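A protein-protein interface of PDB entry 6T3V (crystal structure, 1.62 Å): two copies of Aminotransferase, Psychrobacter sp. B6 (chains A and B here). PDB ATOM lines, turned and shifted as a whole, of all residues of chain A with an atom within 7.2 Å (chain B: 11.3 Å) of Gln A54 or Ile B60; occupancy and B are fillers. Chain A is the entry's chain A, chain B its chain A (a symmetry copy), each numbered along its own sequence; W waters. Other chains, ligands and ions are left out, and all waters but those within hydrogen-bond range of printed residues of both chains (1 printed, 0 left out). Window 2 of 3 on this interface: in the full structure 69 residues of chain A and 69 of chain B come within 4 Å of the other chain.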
ATOM      1  N   VAL A  45      -5.954 -15.611  -5.725  1.00  0.00           N
ATOM      2  CA  VAL A  45      -6.157 -14.256  -5.251  1.00  0.00           C
ATOM      3  C   VAL A  45      -5.840 -14.335  -3.769  1.00  0.00           C
ATOM      4  O   VAL A  45      -6.517 -15.100  -3.026  1.00  0.00           O
ATOM      5  CB  VAL A  45      -7.631 -13.814  -5.444  1.00  0.00           C
ATOM      6  CG1 VAL A  45      -7.832 -12.439  -4.805  1.00  0.00           C
ATOM      7  CG2 VAL A  45      -8.008 -13.770  -6.927  1.00  0.00           C
ATOM      8  N   LEU A  46      -4.823 -13.602  -3.313  1.00  0.00           N
ATOM      9  CA  LEU A  46      -4.479 -13.643  -1.879  1.00  0.00           C
ATOM     10  C   LEU A  46      -5.600 -12.990  -1.045  1.00  0.00           C
ATOM     11  O   LEU A  46      -6.229 -12.012  -1.468  1.00  0.00           O
ATOM     12  CB  LEU A  46      -3.136 -12.963  -1.582  1.00  0.00           C
ATOM     13  CG  LEU A  46      -1.922 -13.482  -2.358  1.00  0.00           C
ATOM     14  CD1 LEU A  46      -0.655 -12.823  -1.788  1.00  0.00           C
ATOM     15  CD2 LEU A  46      -1.818 -14.994  -2.318  1.00  0.00           C
ATOM     16  N   ASP A  47      -5.841 -13.557   0.120  1.00  0.00           N
ATOM     17  CA  ASP A  47      -6.895 -12.979   0.976  1.00  0.00           C
ATOM     18  C   ASP A  47      -6.563 -11.553   1.390  1.00  0.00           C
ATOM     19  O   ASP A  47      -7.499 -10.733   1.508  1.00  0.00           O
ATOM     20  CB  ASP A  47      -7.122 -13.840   2.185  1.00  0.00           C
ATOM     21  CG  ASP A  47      -7.952 -15.056   1.871  1.00  0.00           C
ATOM     22  OD1 ASP A  47      -8.852 -14.972   1.030  1.00  0.00           O
ATOM     23  OD2 ASP A  47      -7.758 -16.083   2.544  1.00  0.00           O
ATOM     24  N   CYS A  48      -5.284 -11.248   1.621  1.00  0.00           N
ATOM     25  CA  CYS A  48      -4.916  -9.875   2.022  1.00  0.00           C
ATOM     26  C   CYS A  48      -5.267  -8.895   0.894  1.00  0.00           C
ATOM     27  O   CYS A  48      -5.747  -7.796   1.158  1.00  0.00           O
ATOM     28  CB  CYS A  48      -3.456  -9.742   2.434  1.00  0.00           C
ATOM     29  SG  CYS A  48      -2.312 -10.355   1.169  1.00  0.00           S
ATOM     30  N   VAL A  49      -5.056  -9.318  -0.350  1.00  0.00           N
ATOM     31  CA  VAL A  49      -5.343  -8.483  -1.520  1.00  0.00           C
ATOM     32  C   VAL A  49      -6.859  -8.343  -1.666  1.00  0.00           C
ATOM     33  O   VAL A  49      -7.336  -7.254  -1.972  1.00  0.00           O
ATOM     34  CB  VAL A  49      -4.724  -9.099  -2.785  1.00  0.00           C
ATOM     35  CG1 VAL A  49      -5.259  -8.417  -4.074  1.00  0.00           C
ATOM     36  CG2 VAL A  49      -3.203  -8.920  -2.699  1.00  0.00           C
ATOM     37  N   LYS A  50      -7.601  -9.442  -1.487  1.00  0.00           N
ATOM     38  CA  LYS A  50      -9.064  -9.364  -1.626  1.00  0.00           C
ATOM     39  C   LYS A  50      -9.606  -8.334  -0.625  1.00  0.00           C
ATOM     40  O   LYS A  50     -10.460  -7.515  -0.973  1.00  0.00           O
ATOM     41  CB  LYS A  50      -9.700 -10.754  -1.394  1.00  0.00           C
ATOM     42  CG  LYS A  50     -11.188 -10.765  -1.701  1.00  0.00           C
ATOM     43  CD  LYS A  50     -11.816 -12.155  -1.524  1.00  0.00           C
ATOM     44  CE  LYS A  50     -13.350 -12.038  -1.577  1.00  0.00           C
ATOM     45  NZ  LYS A  50     -14.033 -13.346  -1.378  1.00  0.00           N
ATOM     46  N   ILE A  51      -9.083  -8.344   0.599  1.00  0.00           N
ATOM     47  CA  ILE A  51      -9.580  -7.357   1.623  1.00  0.00           C
ATOM     48  C   ILE A  51      -9.211  -5.933   1.200  1.00  0.00           C
ATOM     49  O   ILE A  51     -10.051  -4.996   1.267  1.00  0.00           O
ATOM     50  CB  ILE A  51      -9.005  -7.693   3.011  1.00  0.00           C
ATOM     51  CG1 ILE A  51      -9.573  -9.051   3.480  1.00  0.00           C
ATOM     52  CG2 ILE A  51      -9.291  -6.554   4.022  1.00  0.00           C
ATOM     53  CD1 ILE A  51      -8.772  -9.650   4.645  1.00  0.00           C
ATOM     54  N   ALA A  52      -7.960  -5.754   0.735  1.00  0.00           N
ATOM     55  CA  ALA A  52      -7.532  -4.387   0.296  1.00  0.00           C
ATOM     56  C   ALA A  52      -8.414  -3.894  -0.891  1.00  0.00           C
ATOM     57  O   ALA A  52      -8.801  -2.710  -0.940  1.00  0.00           O
ATOM     58  CB  ALA A  52      -6.060  -4.444  -0.129  1.00  0.00           C
ATOM     59  N   GLU A  53      -8.726  -4.780  -1.836  1.00  0.00           N
ATOM     60  CA  GLU A  53      -9.499  -4.382  -3.015  1.00  0.00           C
ATOM     61  C   GLU A  53     -10.936  -4.089  -2.626  1.00  0.00           C
ATOM     62  O   GLU A  53     -11.560  -3.202  -3.219  1.00  0.00           O
ATOM     63  CB  GLU A  53      -9.395  -5.438  -4.130  1.00  0.00           C
ATOM     64  CG  GLU A  53      -7.945  -5.379  -4.664  1.00  0.00           C
ATOM     65  CD  GLU A  53      -7.760  -6.115  -5.973  1.00  0.00           C
ATOM     66  OE1 GLU A  53      -8.221  -7.221  -6.107  1.00  0.00           O
ATOM     67  OE2 GLU A  53      -7.055  -5.619  -6.838  1.00  0.00           O
ATOM     68  N   GLN A  54     -11.477  -4.776  -1.606  1.00  0.00           N
ATOM     69  CA  GLN A  54     -12.829  -4.415  -1.130  1.00  0.00           C
ATOM     70  C   GLN A  54     -12.831  -2.986  -0.561  1.00  0.00           C
ATOM     71  O   GLN A  54     -13.793  -2.230  -0.745  1.00  0.00           O
ATOM     72  CB  GLN A  54     -13.304  -5.440  -0.096  1.00  0.00           C
ATOM     73  CG  GLN A  54     -13.642  -6.801  -0.716  1.00  0.00           C
ATOM     74  CD  GLN A  54     -13.916  -7.862   0.350  1.00  0.00           C
ATOM     75  OE1 GLN A  54     -13.026  -8.621   0.725  1.00  0.00           O
ATOM     76  NE2 GLN A  54     -15.152  -7.908   0.847  1.00  0.00           N
ATOM     77  N   ARG A  55     -11.734  -2.616   0.120  1.00  0.00           N
ATOM     78  CA  ARG A  55     -11.571  -1.249   0.652  1.00  0.00           C
ATOM     79  C   ARG A  55     -11.475  -0.225  -0.482  1.00  0.00           C
ATOM     80  O   ARG A  55     -12.094   0.839  -0.424  1.00  0.00           O
ATOM     81  CB  ARG A  55     -10.358  -1.169   1.601  1.00  0.00           C
ATOM     82  CG  ARG A  55      -9.973   0.249   2.054  1.00  0.00           C
ATOM     83  CD  ARG A  55     -11.052   0.868   2.985  1.00  0.00           C
ATOM     84  NE  ARG A  55     -10.822   2.313   3.218  1.00  0.00           N
ATOM     85  CZ  ARG A  55      -9.854   2.835   3.977  1.00  0.00           C
ATOM     86  NH1 ARG A  55      -8.975   2.067   4.635  1.00  0.00           N
ATOM     87  NH2 ARG A  55      -9.756   4.152   4.071  1.00  0.00           N
ATOM     88  N   ILE A  56     -10.714  -0.545  -1.526  1.00  0.00           N
ATOM     89  CA  ILE A  56     -10.550   0.390  -2.641  1.00  0.00           C
ATOM     90  C   ILE A  56     -11.892   0.588  -3.356  1.00  0.00           C
ATOM     91  O   ILE A  56     -12.143   1.676  -3.871  1.00  0.00           O
ATOM     92  CB  ILE A  56      -9.469  -0.143  -3.610  1.00  0.00           C
ATOM     93  CG1 ILE A  56      -8.107  -0.099  -2.870  1.00  0.00           C
ATOM     94  CG2 ILE A  56      -9.414   0.686  -4.918  1.00  0.00           C
ATOM     95  CD1 ILE A  56      -7.049  -0.942  -3.580  1.00  0.00           C
ATOM     96  N   ALA A  57     -12.746  -0.451  -3.370  1.00  0.00           N
ATOM     97  CA  ALA A  57     -14.035  -0.384  -4.041  1.00  0.00           C
ATOM     98  C   ALA A  57     -15.135   0.259  -3.196  1.00  0.00           C
ATOM     99  O   ALA A  57     -16.263   0.419  -3.696  1.00  0.00           O
ATOM    100  CB  ALA A  57     -14.444  -1.766  -4.515  1.00  0.00           C
ATOM    101  N   ASP A  58     -14.816   0.679  -1.966  1.00  0.00           N
ATOM    102  CA  ASP A  58     -15.852   1.184  -1.023  1.00  0.00           C
ATOM    103  C   ASP A  58     -15.324   2.326  -0.156  1.00  0.00           C
ATOM    104  O   ASP A  58     -14.784   2.091   0.928  1.00  0.00           O
ATOM    105  CB  ASP A  58     -16.466   0.031  -0.221  1.00  0.00           C
ATOM    106  CG  ASP A  58     -17.548   0.520   0.740  1.00  0.00           C
ATOM    107  OD1 ASP A  58     -18.344   1.386   0.307  1.00  0.00           O
ATOM    108  OD2 ASP A  58     -17.533   0.081   1.904  1.00  0.00           O
ATOM    109  N   PRO A  59     -15.424   3.568  -0.642  1.00  0.00           N
ATOM    110  CA  PRO A  59     -16.142   3.906  -1.877  1.00  0.00           C
ATOM    111  C   PRO A  59     -15.225   3.978  -3.075  1.00  0.00           C
ATOM    112  O   PRO A  59     -14.003   4.240  -2.928  1.00  0.00           O
ATOM    113  CB  PRO A  59     -16.636   5.333  -1.586  1.00  0.00           C
ATOM    114  CG  PRO A  59     -15.553   5.899  -0.763  1.00  0.00           C
ATOM    115  CD  PRO A  59     -15.008   4.783   0.082  1.00  0.00           C
ATOM    116  N   HIS A 289      -4.342   1.897  -8.724  1.00  0.00           N
ATOM    117  CA  HIS A 289      -4.996   0.706  -8.086  1.00  0.00           C
ATOM    118  C   HIS A 289      -3.917  -0.197  -7.418  1.00  0.00           C
ATOM    119  O   HIS A 289      -4.020  -0.517  -6.222  1.00  0.00           O
ATOM    120  CB  HIS A 289      -5.723  -0.108  -9.159  1.00  0.00           C
ATOM    121  CG  HIS A 289      -6.520  -1.219  -8.533  1.00  0.00           C
ATOM    122  ND1 HIS A 289      -7.726  -0.982  -7.908  1.00  0.00           N
ATOM    123  CD2 HIS A 289      -6.220  -2.534  -8.336  1.00  0.00           C
ATOM    124  CE1 HIS A 289      -8.164  -2.125  -7.379  1.00  0.00           C
ATOM    125  NE2 HIS A 289      -7.283  -3.076  -7.627  1.00  0.00           N
ATOM    126  N   ALA B  52     -18.149   0.253 -14.399  1.00  0.00           N
ATOM    127  CA  ALA B  52     -17.070  -0.701 -14.811  1.00  0.00           C
ATOM    128  C   ALA B  52     -16.300  -1.224 -13.561  1.00  0.00           C
ATOM    129  O   ALA B  52     -15.964  -2.422 -13.484  1.00  0.00           O
ATOM    130  CB  ALA B  52     -16.108   0.021 -15.761  1.00  0.00           C
ATOM    131  N   GLU B  53     -16.017  -0.347 -12.600  1.00  0.00           N
ATOM    132  CA  GLU B  53     -15.241  -0.744 -11.422  1.00  0.00           C
ATOM    133  C   GLU B  53     -16.066  -1.656 -10.534  1.00  0.00           C
ATOM    134  O   GLU B  53     -15.509  -2.561  -9.903  1.00  0.00           O
ATOM    135  CB  GLU B  53     -14.706   0.486 -10.668  1.00  0.00           C
ATOM    136  CG  GLU B  53     -13.620   1.121 -11.567  1.00  0.00           C
ATOM    137  CD  GLU B  53     -12.767   2.140 -10.844  1.00  0.00           C
ATOM    138  OE1 GLU B  53     -13.293   2.977 -10.152  1.00  0.00           O
ATOM    139  OE2 GLU B  53     -11.566   2.166 -11.055  1.00  0.00           O
ATOM    140  N   GLN B  54     -17.398  -1.481 -10.496  1.00  0.00           N
ATOM    141  CA  GLN B  54     -18.232  -2.439  -9.738  1.00  0.00           C
ATOM    142  C   GLN B  54     -18.132  -3.842 -10.362  1.00  0.00           C
ATOM    143  O   GLN B  54     -18.105  -4.852  -9.650  1.00  0.00           O
ATOM    144  CB  GLN B  54     -19.677  -1.939  -9.687  1.00  0.00           C
ATOM    145  CG  GLN B  54     -19.856  -0.719  -8.775  1.00  0.00           C
ATOM    146  CD  GLN B  54     -21.256  -0.116  -8.896  1.00  0.00           C
ATOM    147  OE1 GLN B  54     -21.470   0.828  -9.653  1.00  0.00           O
ATOM    148  NE2 GLN B  54     -22.214  -0.669  -8.154  1.00  0.00           N
ATOM    149  N   ARG B  55     -18.062  -3.892 -11.702  1.00  0.00           N
ATOM    150  CA  ARG B  55     -17.885  -5.167 -12.426  1.00  0.00           C
ATOM    151  C   ARG B  55     -16.523  -5.791 -12.115  1.00  0.00           C
ATOM    152  O   ARG B  55     -16.423  -6.997 -11.880  1.00  0.00           O
ATOM    153  CB  ARG B  55     -18.095  -4.972 -13.941  1.00  0.00           C
ATOM    154  CG  ARG B  55     -17.738  -6.188 -14.813  1.00  0.00           C
ATOM    155  CD  ARG B  55     -18.720  -7.370 -14.580  1.00  0.00           C
ATOM    156  NE  ARG B  55     -18.242  -8.621 -15.213  1.00  0.00           N
ATOM    157  CZ  ARG B  55     -18.231  -8.875 -16.525  1.00  0.00           C
ATOM    158  NH1 ARG B  55     -18.683  -7.990 -17.424  1.00  0.00           N
ATOM    159  NH2 ARG B  55     -17.748 -10.034 -16.948  1.00  0.00           N
ATOM    160  N   ILE B  56     -15.472  -4.976 -12.095  1.00  0.00           N
ATOM    161  CA  ILE B  56     -14.130  -5.500 -11.830  1.00  0.00           C
ATOM    162  C   ILE B  56     -14.056  -6.045 -10.399  1.00  0.00           C
ATOM    163  O   ILE B  56     -13.321  -7.000 -10.158  1.00  0.00           O
ATOM    164  CB  ILE B  56     -13.084  -4.385 -12.063  1.00  0.00           C
ATOM    165  CG1 ILE B  56     -13.073  -4.054 -13.578  1.00  0.00           C
ATOM    166  CG2 ILE B  56     -11.673  -4.814 -11.582  1.00  0.00           C
ATOM    167  CD1 ILE B  56     -12.368  -2.729 -13.863  1.00  0.00           C
ATOM    168  N   ALA B  57     -14.824  -5.449  -9.469  1.00  0.00           N
ATOM    169  CA  ALA B  57     -14.814  -5.865  -8.075  1.00  0.00           C
ATOM    170  C   ALA B  57     -15.726  -7.059  -7.785  1.00  0.00           C
ATOM    171  O   ALA B  57     -15.749  -7.533  -6.634  1.00  0.00           O
ATOM    172  CB  ALA B  57     -15.151  -4.687  -7.180  1.00  0.00           C
ATOM    173  N   ASP B  58     -16.419  -7.581  -8.804  1.00  0.00           N
ATOM    174  CA  ASP B  58     -17.436  -8.647  -8.587  1.00  0.00           C
ATOM    175  C   ASP B  58     -17.461  -9.651  -9.738  1.00  0.00           C
ATOM    176  O   ASP B  58     -18.198  -9.470 -10.711  1.00  0.00           O
ATOM    177  CB  ASP B  58     -18.805  -8.036  -8.269  1.00  0.00           C
ATOM    178  CG  ASP B  58     -19.863  -9.109  -8.021  1.00  0.00           C
ATOM    179  OD1 ASP B  58     -19.519 -10.099  -7.334  1.00  0.00           O
ATOM    180  OD2 ASP B  58     -20.973  -8.970  -8.567  1.00  0.00           O
ATOM    181  N   PRO B  59     -16.624 -10.692  -9.668  1.00  0.00           N
ATOM    182  CA  PRO B  59     -15.802 -11.002  -8.492  1.00  0.00           C
ATOM    183  C   PRO B  59     -14.404 -10.441  -8.601  1.00  0.00           C
ATOM    184  O   PRO B  59     -13.889 -10.228  -9.729  1.00  0.00           O
ATOM    185  CB  PRO B  59     -15.694 -12.534  -8.566  1.00  0.00           C
ATOM    186  CG  PRO B  59     -15.667 -12.796 -10.014  1.00  0.00           C
ATOM    187  CD  PRO B  59     -16.553 -11.774 -10.668  1.00  0.00           C
ATOM    188  N   ILE B  60     -13.770 -10.269  -7.454  1.00  0.00           N
ATOM    189  CA  ILE B  60     -12.304 -10.017  -7.427  1.00  0.00           C
ATOM    190  C   ILE B  60     -11.607 -11.233  -8.037  1.00  0.00           C
ATOM    191  O   ILE B  60     -11.781 -12.365  -7.580  1.00  0.00           O
ATOM    192  CB  ILE B  60     -11.791  -9.654  -6.014  1.00  0.00           C
ATOM    193  CG1 ILE B  60     -12.338  -8.239  -5.651  1.00  0.00           C
ATOM    194  CG2 ILE B  60     -10.248  -9.695  -5.948  1.00  0.00           C
ATOM    195  CD1 ILE B  60     -12.290  -7.961  -4.164  1.00  0.00           C
ATOM    196  N   SER B  61     -10.845 -10.983  -9.105  1.00  0.00           N
ATOM    197  CA  SER B  61     -10.372 -12.062  -9.978  1.00  0.00           C
ATOM    198  C   SER B  61      -8.853 -12.213  -9.932  1.00  0.00           C
ATOM    199  O   SER B  61      -8.156 -11.284  -9.565  1.00  0.00           O
ATOM    200  CB  SER B  61     -10.784 -11.715 -11.398  1.00  0.00           C
ATOM    201  OG  SER B  61     -12.206 -11.781 -11.502  1.00  0.00           O
ATOM    202  N   PRO B  62      -8.339 -13.394 -10.316  1.00  0.00           N
ATOM    203  CA  PRO B  62      -6.865 -13.551 -10.434  1.00  0.00           C
ATOM    204  C   PRO B  62      -6.290 -12.456 -11.338  1.00  0.00           C
ATOM    205  O   PRO B  62      -7.003 -11.924 -12.199  1.00  0.00           O
ATOM    206  CB  PRO B  62      -6.710 -14.919 -11.081  1.00  0.00           C
ATOM    207  CG  PRO B  62      -7.943 -15.652 -10.606  1.00  0.00           C
ATOM    208  CD  PRO B  62      -9.050 -14.631 -10.670  1.00  0.00           C
ATOM    209  N   ARG B  63      -5.002 -12.161 -11.160  1.00  0.00           N
ATOM    210  CA  ARG B  63      -4.403 -11.017 -11.822  1.00  0.00           C
ATOM    211  C   ARG B  63      -3.144 -11.415 -12.628  1.00  0.00           C
ATOM    212  O   ARG B  63      -2.041 -10.951 -12.321  1.00  0.00           O
ATOM    213  CB  ARG B  63      -4.088  -9.947 -10.775  1.00  0.00           C
ATOM    214  CG  ARG B  63      -4.427  -8.523 -11.257  1.00  0.00           C
ATOM    215  CD  ARG B  63      -5.939  -8.288 -11.576  1.00  0.00           C
ATOM    216  NE  ARG B  63      -6.757  -8.806 -10.425  1.00  0.00           N
ATOM    217  CZ  ARG B  63      -6.878  -8.176  -9.259  1.00  0.00           C
ATOM    218  NH1 ARG B  63      -6.350  -6.969  -9.049  1.00  0.00           N
ATOM    219  NH2 ARG B  63      -7.543  -8.769  -8.233  1.00  0.00           N
ATOM    220  N   PRO B  64      -3.328 -12.232 -13.672  1.00  0.00           N
ATOM    221  CA  PRO B  64      -2.198 -12.541 -14.529  1.00  0.00           C
ATOM    222  C   PRO B  64      -1.694 -11.293 -15.273  1.00  0.00           C
ATOM    223  O   PRO B  64      -2.388 -10.259 -15.355  1.00  0.00           O
ATOM    224  CB  PRO B  64      -2.803 -13.523 -15.550  1.00  0.00           C
ATOM    225  CG  PRO B  64      -4.283 -13.086 -15.619  1.00  0.00           C
ATOM    226  CD  PRO B  64      -4.592 -12.846 -14.172  1.00  0.00           C
ATOM    227  N   SER B 288      -3.485  -3.925 -15.230  1.00  0.00           N
ATOM    228  CA  SER B 288      -4.752  -4.633 -15.395  1.00  0.00           C
ATOM    229  C   SER B 288      -5.955  -3.734 -15.036  1.00  0.00           C
ATOM    230  O   SER B 288      -6.923  -3.732 -15.789  1.00  0.00           O
ATOM    231  CB  SER B 288      -4.757  -5.840 -14.443  1.00  0.00           C
ATOM    232  OG  SER B 288      -5.912  -6.609 -14.667  1.00  0.00           O
ATOM    233  N   HIS B 289      -5.907  -3.061 -13.896  1.00  0.00           N
ATOM    234  CA  HIS B 289      -7.177  -2.397 -13.449  1.00  0.00           C
ATOM    235  C   HIS B 289      -7.602  -1.315 -14.485  1.00  0.00           C
ATOM    236  O   HIS B 289      -8.742  -1.334 -14.980  1.00  0.00           O
ATOM    237  CB  HIS B 289      -6.943  -1.717 -12.097  1.00  0.00           C
ATOM    238  CG  HIS B 289      -8.232  -1.176 -11.544  1.00  0.00           C
ATOM    239  ND1 HIS B 289      -9.170  -2.000 -10.959  1.00  0.00           N
ATOM    240  CD2 HIS B 289      -8.778   0.071 -11.603  1.00  0.00           C
ATOM    241  CE1 HIS B 289     -10.239  -1.268 -10.637  1.00  0.00           C
ATOM    242  NE2 HIS B 289     -10.027  -0.019 -11.006  1.00  0.00           N
ATOM    243  N   ARG B 292      -8.815  -2.852 -17.777  1.00  0.00           N
ATOM    244  CA  ARG B 292     -10.198  -3.408 -17.717  1.00  0.00           C
ATOM    245  C   ARG B 292     -11.220  -2.276 -17.744  1.00  0.00           C
ATOM    246  O   ARG B 292     -12.273  -2.450 -18.378  1.00  0.00           O
ATOM    247  CB  ARG B 292     -10.403  -4.248 -16.462  1.00  0.00           C
ATOM    248  CG  ARG B 292      -9.729  -5.619 -16.539  1.00  0.00           C
ATOM    249  CD  ARG B 292     -10.412  -6.626 -15.578  1.00  0.00           C
ATOM    250  NE  ARG B 292     -11.817  -6.964 -15.944  1.00  0.00           N
ATOM    251  CZ  ARG B 292     -12.662  -7.635 -15.135  1.00  0.00           C
ATOM    252  NH1 ARG B 292     -12.311  -8.027 -13.895  1.00  0.00           N
ATOM    253  NH2 ARG B 292     -13.899  -7.891 -15.544  1.00  0.00           N
HETATM  254  O   HOH W   1      -9.595  -6.035  -8.880  1.00  0.00           O
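Water W1 lies within hydrogen-bond range of the side-chain carboxylate (OE2) of Glu A53 and the guanidinium group (NH1) of Arg B63.
The side-chain carboxylate of Glu A53 lies within salt-bridge range of the guanidinium group of Arg B63.
Among the printed residues, pairs that only touch across the chains: Glu A53 with Ile B60, Val A45 with Pro B62, His A289 with His B289, Val A45 with Ser B61, Lys A50 with Ile B60, Val A45 with Ile B60 and Gln A54 with Ile B60.
OE1 of Gln A54 sits close to O of Lys A50, at 3.3 Å. A ring nitrogen (NE2) of His A289 is in hydrogen-bond range of the side-chain carboxylate of Glu A53. The side-chain carboxylate of Glu B53 lies within hydrogen-bond range of a ring nitrogen (NE2) of His B289, at 2.7 Å. OG of Ser B61 sits at hydrogen-bond distance from O of Pro B59 (2.9 Å). The guanidinium group (NH2) of Arg B63 is in hydrogen-bond range of the backbone carbonyl oxygen (O) of Ser B61 (2.9 Å).
Printed residues of chain B within 4 Å of Gln A54: Ile B60 (3.9 Å). Of the printed residues of chain A, Ile B60 touches Val A45, Lys A50, Glu A53 and Gln A54. Val A45 touches just these residues of chain B: Ile B60, Ser B61 and Pro B62. No residue of chain B comes within 4 Å of Ile A51. Ala A52 touches none of the printed residues of chain B. Glu A53 touches just these residues of chain B: Ile B60 and Arg B63. No residue of chain B comes within 4 Å of Ile A56. Printed residues of chain A within 4 Å of His B289: His A289 (3.5 Å). Printed residues of chain A within 4 Å of Ser B61: Val A45 (3.5 Å). Of the printed residues of chain B, His A289 touches His B289 (3.5 Å). Printed residues of chain A within 4 Å of Arg B63: Glu A53. The nearest printed residue of chain B that does not touch Gln A54 is Ala B57 (6.3 Å).
Of the 16 printed residues of chain A, 5 touch a printed residue of chain B. Hydrophobic or aromatic side chains of chain B within 4 Å of the printed part of chain A: Ile B60, Pro B62 and His B289. Among the printed residues, 8 pairs touch across the chains.
His A289 touches its own counterpart, His B289. 9 positions are printed for both chains. Of the 8 pairs that touch across the chains among the printed residues, 1 has its exchanged pair printed and touching as well.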
